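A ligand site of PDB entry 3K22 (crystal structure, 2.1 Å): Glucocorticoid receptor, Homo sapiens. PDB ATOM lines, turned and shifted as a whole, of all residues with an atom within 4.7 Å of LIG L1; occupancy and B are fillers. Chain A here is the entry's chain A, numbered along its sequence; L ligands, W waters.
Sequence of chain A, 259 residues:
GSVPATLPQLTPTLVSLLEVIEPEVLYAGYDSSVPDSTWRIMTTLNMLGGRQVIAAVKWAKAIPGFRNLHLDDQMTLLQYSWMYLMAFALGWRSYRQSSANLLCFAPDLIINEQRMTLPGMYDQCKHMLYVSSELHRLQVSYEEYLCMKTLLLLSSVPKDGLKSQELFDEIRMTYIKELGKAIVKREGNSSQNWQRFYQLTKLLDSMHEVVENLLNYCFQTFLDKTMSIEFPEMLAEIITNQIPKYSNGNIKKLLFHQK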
ATOM      1  N   GLU A  22     -20.967  -7.947 -30.653  1.00  0.00           N
ATOM      2  CA  GLU A  22     -20.453  -6.840 -29.836  1.00  0.00           C
ATOM      3  C   GLU A  22     -19.029  -7.137 -29.406  1.00  0.00           C
ATOM      4  O   GLU A  22     -18.804  -8.160 -28.759  1.00  0.00           O
ATOM      5  CB  GLU A  22     -21.341  -6.623 -28.596  1.00  0.00           C
ATOM      6  CG  GLU A  22     -20.936  -5.463 -27.689  1.00  0.00           C
ATOM      7  CD  GLU A  22     -20.903  -4.110 -28.386  1.00  0.00           C
ATOM      8  OE1 GLU A  22     -21.638  -3.896 -29.384  1.00  0.00           O
ATOM      9  OE2 GLU A  22     -20.130  -3.231 -27.935  1.00  0.00           O
ATOM     10  N   PRO A  23     -18.071  -6.259 -29.746  1.00  0.00           N
ATOM     11  CA  PRO A  23     -16.653  -6.512 -29.488  1.00  0.00           C
ATOM     12  C   PRO A  23     -16.297  -6.798 -28.021  1.00  0.00           C
ATOM     13  O   PRO A  23     -16.923  -6.270 -27.102  1.00  0.00           O
ATOM     14  CB  PRO A  23     -15.967  -5.222 -29.941  1.00  0.00           C
ATOM     15  CG  PRO A  23     -16.881  -4.619 -30.913  1.00  0.00           C
ATOM     16  CD  PRO A  23     -18.245  -4.961 -30.436  1.00  0.00           C
ATOM     17  N   MET A  42      -2.201   9.777 -22.319  1.00  0.00           N
ATOM     18  CA  MET A  42      -2.366  10.166 -23.712  1.00  0.00           C
ATOM     19  C   MET A  42      -1.864   9.069 -24.652  1.00  0.00           C
ATOM     20  O   MET A  42      -2.553   8.654 -25.585  1.00  0.00           O
ATOM     21  CB  MET A  42      -1.616  11.487 -24.002  1.00  0.00           C
ATOM     22  CG  MET A  42      -2.284  12.744 -23.441  1.00  0.00           C
ATOM     23  SD  MET A  42      -1.439  14.326 -23.833  1.00  0.00           S
ATOM     24  CE  MET A  42      -0.375  14.596 -22.418  1.00  0.00           C
ATOM     25  N   LEU A  45      -3.962   5.712 -24.500  1.00  0.00           N
ATOM     26  CA  LEU A  45      -5.297   5.855 -25.087  1.00  0.00           C
ATOM     27  C   LEU A  45      -5.251   5.945 -26.612  1.00  0.00           C
ATOM     28  O   LEU A  45      -6.183   5.515 -27.286  1.00  0.00           O
ATOM     29  CB  LEU A  45      -6.014   7.083 -24.507  1.00  0.00           C
ATOM     30  CG  LEU A  45      -6.447   6.961 -23.042  1.00  0.00           C
ATOM     31  CD1 LEU A  45      -6.893   8.306 -22.481  1.00  0.00           C
ATOM     32  CD2 LEU A  45      -7.550   5.931 -22.918  1.00  0.00           C
ATOM     33  N   ASN A  46      -4.182   6.532 -27.137  1.00  0.00           N
ATOM     34  CA  ASN A  46      -3.918   6.483 -28.576  1.00  0.00           C
ATOM     35  C   ASN A  46      -3.766   5.048 -29.041  1.00  0.00           C
ATOM     36  O   ASN A  46      -4.375   4.649 -30.028  1.00  0.00           O
ATOM     37  CB  ASN A  46      -2.637   7.251 -28.930  1.00  0.00           C
ATOM     38  CG  ASN A  46      -2.826   8.753 -28.887  1.00  0.00           C
ATOM     39  OD1 ASN A  46      -3.910   9.243 -28.567  1.00  0.00           O
ATOM     40  ND2 ASN A  46      -1.780   9.482 -29.229  1.00  0.00           N
ATOM     41  N   LEU A  48      -4.679   2.176 -27.408  1.00  0.00           N
ATOM     42  CA  LEU A  48      -5.922   1.448 -27.181  1.00  0.00           C
ATOM     43  C   LEU A  48      -6.943   1.804 -28.252  1.00  0.00           C
ATOM     44  O   LEU A  48      -7.656   0.944 -28.755  1.00  0.00           O
ATOM     45  CB  LEU A  48      -6.490   1.759 -25.774  1.00  0.00           C
ATOM     46  CG  LEU A  48      -7.797   1.067 -25.351  1.00  0.00           C
ATOM     47  CD1 LEU A  48      -7.693  -0.460 -25.411  1.00  0.00           C
ATOM     48  CD2 LEU A  48      -8.201   1.524 -23.947  1.00  0.00           C
ATOM     49  N   GLY A  49      -6.983   3.081 -28.605  1.00  0.00           N
ATOM     50  CA  GLY A  49      -7.891   3.598 -29.617  1.00  0.00           C
ATOM     51  C   GLY A  49      -7.692   2.944 -30.960  1.00  0.00           C
ATOM     52  O   GLY A  49      -8.651   2.691 -31.687  1.00  0.00           O
ATOM     53  N   GLN A  52      -9.094  -0.716 -30.886  1.00  0.00           N
ATOM     54  CA  GLN A  52     -10.540  -0.790 -30.812  1.00  0.00           C
ATOM     55  C   GLN A  52     -11.222  -0.384 -32.095  1.00  0.00           C
ATOM     56  O   GLN A  52     -12.292  -0.866 -32.405  1.00  0.00           O
ATOM     57  CB  GLN A  52     -11.058   0.034 -29.637  1.00  0.00           C
ATOM     58  CG  GLN A  52     -11.779  -0.805 -28.615  1.00  0.00           C
ATOM     59  CD  GLN A  52     -11.514  -0.331 -27.215  1.00  0.00           C
ATOM     60  OE1 GLN A  52     -11.921  -0.965 -26.249  1.00  0.00           O
ATOM     61  NE2 GLN A  52     -10.827   0.782 -27.104  1.00  0.00           N
ATOM     62  N   ALA A  55     -11.052  -3.470 -33.832  1.00  0.00           N
ATOM     63  CA  ALA A  55     -12.172  -4.254 -33.319  1.00  0.00           C
ATOM     64  C   ALA A  55     -13.477  -3.823 -33.986  1.00  0.00           C
ATOM     65  O   ALA A  55     -14.305  -4.664 -34.336  1.00  0.00           O
ATOM     66  CB  ALA A  55     -12.283  -4.084 -31.832  1.00  0.00           C
ATOM     67  N   ALA A  56     -13.648  -2.521 -34.176  1.00  0.00           N
ATOM     68  CA  ALA A  56     -14.849  -1.964 -34.796  1.00  0.00           C
ATOM     69  C   ALA A  56     -14.994  -2.385 -36.249  1.00  0.00           C
ATOM     70  O   ALA A  56     -16.123  -2.592 -36.720  1.00  0.00           O
ATOM     71  CB  ALA A  56     -14.830  -0.439 -34.690  1.00  0.00           C
ATOM     72  N   TRP A  82     -15.542   6.458 -36.592  1.00  0.00           N
ATOM     73  CA  TRP A  82     -14.776   5.736 -35.556  1.00  0.00           C
ATOM     74  C   TRP A  82     -14.854   6.388 -34.166  1.00  0.00           C
ATOM     75  O   TRP A  82     -15.050   5.696 -33.163  1.00  0.00           O
ATOM     76  CB  TRP A  82     -13.320   5.470 -35.984  1.00  0.00           C
ATOM     77  CG  TRP A  82     -12.513   6.680 -36.232  1.00  0.00           C
ATOM     78  CD1 TRP A  82     -12.451   7.398 -37.380  1.00  0.00           C
ATOM     79  CD2 TRP A  82     -11.638   7.333 -35.299  1.00  0.00           C
ATOM     80  NE1 TRP A  82     -11.601   8.468 -37.234  1.00  0.00           N
ATOM     81  CE2 TRP A  82     -11.085   8.451 -35.961  1.00  0.00           C
ATOM     82  CE3 TRP A  82     -11.271   7.085 -33.978  1.00  0.00           C
ATOM     83  CZ2 TRP A  82     -10.181   9.321 -35.341  1.00  0.00           C
ATOM     84  CZ3 TRP A  82     -10.367   7.956 -33.358  1.00  0.00           C
ATOM     85  CH2 TRP A  82      -9.839   9.058 -34.048  1.00  0.00           C
ATOM     86  N   MET A  83     -14.750   7.717 -34.114  1.00  0.00           N
ATOM     87  CA  MET A  83     -14.799   8.440 -32.826  1.00  0.00           C
ATOM     88  C   MET A  83     -16.199   8.417 -32.217  1.00  0.00           C
ATOM     89  O   MET A  83     -16.324   8.385 -30.988  1.00  0.00           O
ATOM     90  CB  MET A  83     -14.318   9.879 -32.979  1.00  0.00           C
ATOM     91  CG  MET A  83     -14.169  10.642 -31.649  1.00  0.00           C
ATOM     92  SD  MET A  83     -12.926   9.959 -30.520  1.00  0.00           S
ATOM     93  CE  MET A  83     -11.413  10.557 -31.270  1.00  0.00           C
ATOM     94  N   LEU A  85     -18.223   5.888 -32.432  1.00  0.00           N
ATOM     95  CA  LEU A  85     -18.353   4.556 -31.844  1.00  0.00           C
ATOM     96  C   LEU A  85     -17.569   4.461 -30.534  1.00  0.00           C
ATOM     97  O   LEU A  85     -18.066   3.894 -29.563  1.00  0.00           O
ATOM     98  CB  LEU A  85     -17.865   3.482 -32.815  1.00  0.00           C
ATOM     99  CG  LEU A  85     -18.537   3.429 -34.183  1.00  0.00           C
ATOM    100  CD1 LEU A  85     -17.776   2.464 -35.095  1.00  0.00           C
ATOM    101  CD2 LEU A  85     -20.008   3.045 -34.065  1.00  0.00           C
ATOM    102  N   MET A  86     -16.356   4.990 -30.529  1.00  0.00           N
ATOM    103  CA  MET A  86     -15.526   4.994 -29.327  1.00  0.00           C
ATOM    104  C   MET A  86     -16.162   5.834 -28.217  1.00  0.00           C
ATOM    105  O   MET A  86     -16.279   5.369 -27.090  1.00  0.00           O
ATOM    106  CB  MET A  86     -14.119   5.503 -29.613  1.00  0.00           C
ATOM    107  CG  MET A  86     -13.355   4.714 -30.641  1.00  0.00           C
ATOM    108  SD  MET A  86     -11.582   4.787 -30.368  1.00  0.00           S
ATOM    109  CE  MET A  86     -11.341   3.151 -29.688  1.00  0.00           C
ATOM    110  N   ALA A  87     -16.575   7.047 -28.559  1.00  0.00           N
ATOM    111  CA  ALA A  87     -17.285   7.910 -27.615  1.00  0.00           C
ATOM    112  C   ALA A  87     -18.518   7.233 -27.008  1.00  0.00           C
ATOM    113  O   ALA A  87     -18.745   7.313 -25.798  1.00  0.00           O
ATOM    114  CB  ALA A  87     -17.698   9.200 -28.296  1.00  0.00           C
ATOM    115  N   ALA A  89     -19.356   3.891 -26.928  1.00  0.00           N
ATOM    116  CA  ALA A  89     -19.016   2.666 -26.203  1.00  0.00           C
ATOM    117  C   ALA A  89     -18.365   2.995 -24.873  1.00  0.00           C
ATOM    118  O   ALA A  89     -18.538   2.272 -23.894  1.00  0.00           O
ATOM    119  CB  ALA A  89     -18.116   1.791 -27.037  1.00  0.00           C
ATOM    120  N   LEU A  90     -17.596   4.082 -24.848  1.00  0.00           N
ATOM    121  CA  LEU A  90     -16.942   4.563 -23.641  1.00  0.00           C
ATOM    122  C   LEU A  90     -17.994   5.093 -22.656  1.00  0.00           C
ATOM    123  O   LEU A  90     -17.926   4.813 -21.467  1.00  0.00           O
ATOM    124  CB  LEU A  90     -15.927   5.663 -23.955  1.00  0.00           C
ATOM    125  CG  LEU A  90     -15.250   6.283 -22.730  1.00  0.00           C
ATOM    126  CD1 LEU A  90     -14.441   5.229 -21.971  1.00  0.00           C
ATOM    127  CD2 LEU A  90     -14.393   7.486 -23.119  1.00  0.00           C
ATOM    128  N   ARG A  93     -19.865   1.934 -21.201  1.00  0.00           N
ATOM    129  CA  ARG A  93     -19.120   1.197 -20.185  1.00  0.00           C
ATOM    130  C   ARG A  93     -18.987   1.974 -18.884  1.00  0.00           C
ATOM    131  O   ARG A  93     -19.033   1.389 -17.813  1.00  0.00           O
ATOM    132  CB  ARG A  93     -17.725   0.773 -20.675  1.00  0.00           C
ATOM    133  CG  ARG A  93     -17.676  -0.651 -21.216  1.00  0.00           C
ATOM    134  CD  ARG A  93     -16.485  -1.460 -20.667  1.00  0.00           C
ATOM    135  NE  ARG A  93     -15.200  -1.120 -21.287  1.00  0.00           N
ATOM    136  CZ  ARG A  93     -14.867  -1.410 -22.551  1.00  0.00           C
ATOM    137  NH1 ARG A  93     -13.664  -1.061 -23.005  1.00  0.00           N
ATOM    138  NH2 ARG A  93     -15.714  -2.032 -23.370  1.00  0.00           N
ATOM    139  N   PHE A 105     -12.181   3.481 -19.576  1.00  0.00           N
ATOM    140  CA  PHE A 105     -11.576   3.149 -20.866  1.00  0.00           C
ATOM    141  C   PHE A 105     -11.293   1.661 -20.999  1.00  0.00           C
ATOM    142  O   PHE A 105     -11.488   1.077 -22.070  1.00  0.00           O
ATOM    143  CB  PHE A 105     -10.294   3.941 -21.071  1.00  0.00           C
ATOM    144  CG  PHE A 105     -10.535   5.367 -21.437  1.00  0.00           C
ATOM    145  CD1 PHE A 105     -10.532   6.364 -20.477  1.00  0.00           C
ATOM    146  CD2 PHE A 105     -10.779   5.714 -22.760  1.00  0.00           C
ATOM    147  CE1 PHE A 105     -10.749   7.686 -20.829  1.00  0.00           C
ATOM    148  CE2 PHE A 105     -10.993   7.032 -23.125  1.00  0.00           C
ATOM    149  CZ  PHE A 105     -10.986   8.020 -22.154  1.00  0.00           C
ATOM    150  N   MET A 128     -16.916  13.291 -23.008  1.00  0.00           N
ATOM    151  CA  MET A 128     -17.228  11.875 -22.916  1.00  0.00           C
ATOM    152  C   MET A 128     -18.102  11.635 -21.686  1.00  0.00           C
ATOM    153  O   MET A 128     -18.952  10.744 -21.687  1.00  0.00           O
ATOM    154  CB  MET A 128     -15.951  11.056 -22.847  1.00  0.00           C
ATOM    155  CG  MET A 128     -14.964  11.338 -23.994  1.00  0.00           C
ATOM    156  SD  MET A 128     -13.275  10.843 -23.618  1.00  0.00           S
ATOM    157  CE  MET A 128     -12.330  12.232 -24.257  1.00  0.00           C
ATOM    158  N   TYR A 145     -28.877   0.333 -26.593  1.00  0.00           N
ATOM    159  CA  TYR A 145     -27.489   0.714 -26.826  1.00  0.00           C
ATOM    160  C   TYR A 145     -26.916   0.106 -28.100  1.00  0.00           C
ATOM    161  O   TYR A 145     -26.207   0.787 -28.849  1.00  0.00           O
ATOM    162  CB  TYR A 145     -26.645   0.321 -25.608  1.00  0.00           C
ATOM    163  CG  TYR A 145     -25.174   0.151 -25.885  1.00  0.00           C
ATOM    164  CD1 TYR A 145     -24.357   1.258 -26.122  1.00  0.00           C
ATOM    165  CD2 TYR A 145     -24.590  -1.106 -25.890  1.00  0.00           C
ATOM    166  CE1 TYR A 145     -23.012   1.103 -26.368  1.00  0.00           C
ATOM    167  CE2 TYR A 145     -23.245  -1.260 -26.136  1.00  0.00           C
ATOM    168  CZ  TYR A 145     -22.451  -0.159 -26.365  1.00  0.00           C
ATOM    169  OH  TYR A 145     -21.122  -0.317 -26.597  1.00  0.00           O
ATOM    170  N   LYS A 149     -25.530   2.243 -31.225  1.00  0.00           N
ATOM    171  CA  LYS A 149     -24.154   2.215 -31.702  1.00  0.00           C
ATOM    172  C   LYS A 149     -24.137   1.856 -33.192  1.00  0.00           C
ATOM    173  O   LYS A 149     -23.387   2.459 -33.971  1.00  0.00           O
ATOM    174  CB  LYS A 149     -23.289   1.253 -30.890  1.00  0.00           C
ATOM    175  CG  LYS A 149     -21.799   1.341 -31.248  1.00  0.00           C
ATOM    176  CD  LYS A 149     -20.877   0.833 -30.133  1.00  0.00           C
ATOM    177  CE  LYS A 149     -21.112  -0.628 -29.771  1.00  0.00           C
ATOM    178  NZ  LYS A 149     -20.871  -1.565 -30.884  1.00  0.00           N
ATOM    179  N   LEU A 214     -14.059  16.119 -29.721  1.00  0.00           N
ATOM    180  CA  LEU A 214     -13.040  15.080 -29.583  1.00  0.00           C
ATOM    181  C   LEU A 214     -12.096  15.016 -30.783  1.00  0.00           C
ATOM    182  O   LEU A 214     -10.887  14.835 -30.619  1.00  0.00           O
ATOM    183  CB  LEU A 214     -13.701  13.708 -29.392  1.00  0.00           C
ATOM    184  CG  LEU A 214     -14.545  13.535 -28.135  1.00  0.00           C
ATOM    185  CD1 LEU A 214     -15.287  12.229 -28.177  1.00  0.00           C
ATOM    186  CD2 LEU A 214     -13.678  13.631 -26.891  1.00  0.00           C
ATOM    187  N   TYR A 217      -9.572  18.021 -30.903  1.00  0.00           N
ATOM    188  CA  TYR A 217      -8.470  17.753 -29.992  1.00  0.00           C
ATOM    189  C   TYR A 217      -7.505  16.735 -30.578  1.00  0.00           C
ATOM    190  O   TYR A 217      -6.291  16.959 -30.603  1.00  0.00           O
ATOM    191  CB  TYR A 217      -8.972  17.219 -28.636  1.00  0.00           C
ATOM    192  CG  TYR A 217      -7.845  16.671 -27.805  1.00  0.00           C
ATOM    193  CD1 TYR A 217      -6.927  17.518 -27.190  1.00  0.00           C
ATOM    194  CD2 TYR A 217      -7.659  15.290 -27.662  1.00  0.00           C
ATOM    195  CE1 TYR A 217      -5.871  17.022 -26.429  1.00  0.00           C
ATOM    196  CE2 TYR A 217      -6.612  14.774 -26.903  1.00  0.00           C
ATOM    197  CZ  TYR A 217      -5.719  15.651 -26.301  1.00  0.00           C
ATOM    198  OH  TYR A 217      -4.681  15.150 -25.563  1.00  0.00           O
ATOM    199  N   CYS A 218      -8.054  15.616 -31.030  1.00  0.00           N
ATOM    200  CA  CYS A 218      -7.275  14.528 -31.609  1.00  0.00           C
ATOM    201  C   CYS A 218      -6.405  15.012 -32.768  1.00  0.00           C
ATOM    202  O   CYS A 218      -5.228  14.660 -32.868  1.00  0.00           O
ATOM    203  CB  CYS A 218      -8.199  13.419 -32.088  1.00  0.00           C
ATOM    204  SG  CYS A 218      -7.338  12.074 -32.926  1.00  0.00           S
ATOM    205  N   PHE A 231       1.120   7.728 -32.141  1.00  0.00           N
ATOM    206  CA  PHE A 231      -0.156   7.177 -32.595  1.00  0.00           C
ATOM    207  C   PHE A 231       0.072   5.842 -33.322  1.00  0.00           C
ATOM    208  O   PHE A 231       1.082   5.681 -34.011  1.00  0.00           O
ATOM    209  CB  PHE A 231      -0.847   8.143 -33.558  1.00  0.00           C
ATOM    210  CG  PHE A 231      -1.534   9.286 -32.895  1.00  0.00           C
ATOM    211  CD1 PHE A 231      -0.897  10.517 -32.768  1.00  0.00           C
ATOM    212  CD2 PHE A 231      -2.837   9.158 -32.419  1.00  0.00           C
ATOM    213  CE1 PHE A 231      -1.551  11.594 -32.169  1.00  0.00           C
ATOM    214  CE2 PHE A 231      -3.486  10.227 -31.810  1.00  0.00           C
ATOM    215  CZ  PHE A 231      -2.843  11.445 -31.685  1.00  0.00           C
ATOM    216  N   LEU A 235      -4.613   3.882 -37.109  1.00  0.00           N
ATOM    217  CA  LEU A 235      -5.330   5.103 -36.721  1.00  0.00           C
ATOM    218  C   LEU A 235      -4.703   6.368 -37.316  1.00  0.00           C
ATOM    219  O   LEU A 235      -5.412   7.316 -37.655  1.00  0.00           O
ATOM    220  CB  LEU A 235      -5.388   5.218 -35.188  1.00  0.00           C
ATOM    221  CG  LEU A 235      -6.683   5.746 -34.591  1.00  0.00           C
ATOM    222  CD1 LEU A 235      -6.526   5.885 -33.091  1.00  0.00           C
ATOM    223  CD2 LEU A 235      -7.089   7.065 -35.206  1.00  0.00           C
HETATM  224  C1  LIG L   1     -17.294  -1.369 -28.668  1.00  0.00           C
HETATM  225  F1  LIG L   1      -7.489   7.127 -29.751  1.00  0.00           F
HETATM  226  N1  LIG L   1     -15.406   0.074 -28.205  1.00  0.00           N
HETATM  227  O1  LIG L   1     -14.807   2.007 -29.285  1.00  0.00           O
HETATM  228  C2  LIG L   1     -16.379  -0.309 -29.191  1.00  0.00           C
HETATM  229  F2  LIG L   1      -6.167   8.691 -30.452  1.00  0.00           F
HETATM  230  N2  LIG L   1     -11.467   3.983 -26.128  1.00  0.00           N
HETATM  231  O2  LIG L   1      -6.373   8.574 -27.696  1.00  0.00           O
HETATM  232  C3  LIG L   1     -14.815   1.296 -28.297  1.00  0.00           C
HETATM  233  F3  LIG L   1      -8.306   8.943 -30.642  1.00  0.00           F
HETATM  234  N3  LIG L   1     -10.225   3.505 -26.164  1.00  0.00           N
HETATM  235  O3  LIG L   1     -16.099  -1.141 -31.402  1.00  0.00           O
HETATM  236  C4  LIG L   1     -14.156   1.755 -27.091  1.00  0.00           C
HETATM  237  F4  LIG L   1      -6.222  10.806 -29.542  1.00  0.00           F
HETATM  238  N4  LIG L   1      -8.674   7.458 -27.292  1.00  0.00           N
HETATM  239  C5  LIG L   1     -14.553   1.269 -25.879  1.00  0.00           C
HETATM  240  F5  LIG L   1      -6.789  11.103 -27.487  1.00  0.00           F
HETATM  241  N5  LIG L   1     -14.314  -1.151 -29.973  1.00  0.00           N
HETATM  242  C6  LIG L   1     -13.922   1.712 -24.737  1.00  0.00           C
HETATM  243  F6  LIG L   1      -8.287  11.190 -29.055  1.00  0.00           F
HETATM  244  C7  LIG L   1     -12.892   2.613 -24.829  1.00  0.00           C
HETATM  245  C8  LIG L   1     -12.514   3.086 -26.062  1.00  0.00           C
HETATM  246  C9  LIG L   1     -13.130   2.661 -27.207  1.00  0.00           C
HETATM  247  C10 LIG L   1      -9.481   4.556 -26.511  1.00  0.00           C
HETATM  248  C11 LIG L   1     -10.255   5.710 -26.684  1.00  0.00           C
HETATM  249  C12 LIG L   1      -9.972   7.012 -27.027  1.00  0.00           C
HETATM  250  C13 LIG L   1      -8.726   8.801 -27.816  1.00  0.00           C
HETATM  251  C14 LIG L   1      -7.407   9.098 -28.494  1.00  0.00           C
HETATM  252  C15 LIG L   1      -7.340   8.457 -29.851  1.00  0.00           C
HETATM  253  C16 LIG L   1      -7.182  10.562 -28.642  1.00  0.00           C
HETATM  254  C17 LIG L   1     -11.055   7.851 -27.087  1.00  0.00           C
HETATM  255  C18 LIG L   1     -12.329   7.433 -26.821  1.00  0.00           C
HETATM  256  C19 LIG L   1     -13.439   8.403 -26.911  1.00  0.00           C
HETATM  257  C20 LIG L   1     -12.625   6.142 -26.483  1.00  0.00           C
HETATM  258  C21 LIG L   1     -11.540   5.313 -26.427  1.00  0.00           C
HETATM  259  C22 LIG L   1     -15.605  -0.908 -30.316  1.00  0.00           C
HETATM  260  C1  LG2 L   2      -3.370  17.583 -22.879  1.00  0.00           C
HETATM  261  O1  LG2 L   2      -4.102  16.348 -22.995  1.00  0.00           O
HETATM  262  C2  LG2 L   2      -3.062  18.407 -24.128  1.00  0.00           C
HETATM  263  O2  LG2 L   2      -2.927  17.577 -25.281  1.00  0.00           O
HETATM  264  C3  LG2 L   2      -1.763  19.169 -23.940  1.00  0.00           C
HETATM  265  O3  LG2 L   2      -1.530  20.035 -25.047  1.00  0.00           O
HETATM  266  C4  LG2 L   2      -1.873  19.956 -22.642  1.00  0.00           C
HETATM  267  O4  LG2 L   2      -0.745  20.832 -22.497  1.00  0.00           O
HETATM  268  C5  LG2 L   2      -1.967  18.986 -21.470  1.00  0.00           C
HETATM  269  O5  LG2 L   2      -3.119  18.145 -21.577  1.00  0.00           O
HETATM  270  C6  LG2 L   2      -2.008  19.725 -20.126  1.00  0.00           C
HETATM  271  O6  LG2 L   2      -3.182  20.538 -20.032  1.00  0.00           O
HETATM  272  C7  LG2 L   2      -5.064  16.067 -21.971  1.00  0.00           C
HETATM  273  C8  LG2 L   2      -5.302  14.554 -21.854  1.00  0.00           C
HETATM  274  C9  LG2 L   2      -6.206  13.998 -22.964  1.00  0.00           C
HETATM  275  C10 LG2 L   2      -7.274  13.053 -22.407  1.00  0.00           C
HETATM  276  C11 LG2 L   2      -7.728  11.987 -23.409  1.00  0.00           C
HETATM  277  C12 LG2 L   2      -8.960  12.393 -24.194  1.00  0.00           C
HETATM  278  O   HOH W   1     -18.725  -0.777 -32.056  1.00  0.00           O
HETATM  279  O   HOH W   2     -17.891  -4.087 -26.567  1.00  0.00           O
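Water W1 bridges NZ of Lys 149 (2.6 Å) and O3 of LIG L1 (2.7 Å).
Water W2 bridges the backbone carbonyl oxygen of Pro 23 (2.4 Å) and the side-chain carboxylate of Glu 22 (2.8 Å).
SG of Cys 218 lies close to F4 of LIG L1 (3.8 Å).
OE2 of Glu 22 touches C1 of LIG L1, at 3.5 Å.
CG of Pro 23 touches O3 of LIG L1, at 3.6 Å.
CG of Leu 48 touches N3 of LIG L1, at 3.5 Å.
CA of Gly 49 touches F1 of LIG L1, at 3.6 Å.
Ala 56 touches LIG L1 (CB to O3, 3.6 Å).
CZ3 of Trp 82 touches F3 of LIG L1, 3.5 Å away.
CE of Met 83 touches F3 of LIG L1, at 3.6 Å.
Leu 85 touches LIG L1 (O to O1, 3.8 Å).
Met 86 touches LIG L1.
Ala 87 touches LIG L1 (N to C19, 3.8 Å).
CB of Ala 89 touches N1 of LIG L1, 3.4 Å away.
Arg 93 touches LIG L1.
O of Phe 105 touches C7 of LIG L1, 3.5 Å away.
CE2 of Tyr 217 touches F5 of LIG L1, at 3.7 Å.
Phe 231 touches LIG L1 (CE2 to F2, 3.4 Å).
CD1 of Leu 235 touches F1 of LIG L1, at 3.7 Å.
Of the 27 residues printed, 20 come within 4 Å of LIG L1.
The nearest printed residue that does not touch LIG L1 is Leu 90 (4.02 Å).
The backbone carbonyl oxygen of Gln 52 lies close to a nitrogen (N5) of LIG L1.
NE2 of Gln 52 lies within hydrogen-bond range of N3 of LIG L1.
An oxygen (O2) of LIG L1 lies within hydrogen-bond range of the side-chain amide oxygen (OD1) of Asn 46 (2.7 Å).
The backbone carbonyl oxygen of Leu 45 sits close to an oxygen (O2) of LIG L1, at 3.1 Å.
O1 of LG2 L2 lies within hydrogen-bond range of OH of Tyr 217 (2.9 Å).
The backbone NH of Asn 46 is in hydrogen-bond range of an oxygen (O2) of LIG L1, at 3.0 Å.
O of Phe 105 sits at hydrogen-bond distance from NH1 of Arg 93 (3.2 Å).
OD1 of Asn 46 lies close to O of Met 42 (3.3 Å).
SD of Met 42 lies within hydrogen-bond range of OH of Tyr 217 (3.8 Å).
The side-chain carboxylate of Glu 22 sits at hydrogen-bond distance from the side-chain hydroxyl of Tyr 145 (3.4 Å).
The side-chain carboxylate (OE1) of Glu 22 lies within salt-bridge range of the side-chain amino group (NZ) of Lys 149 (2.9 Å).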
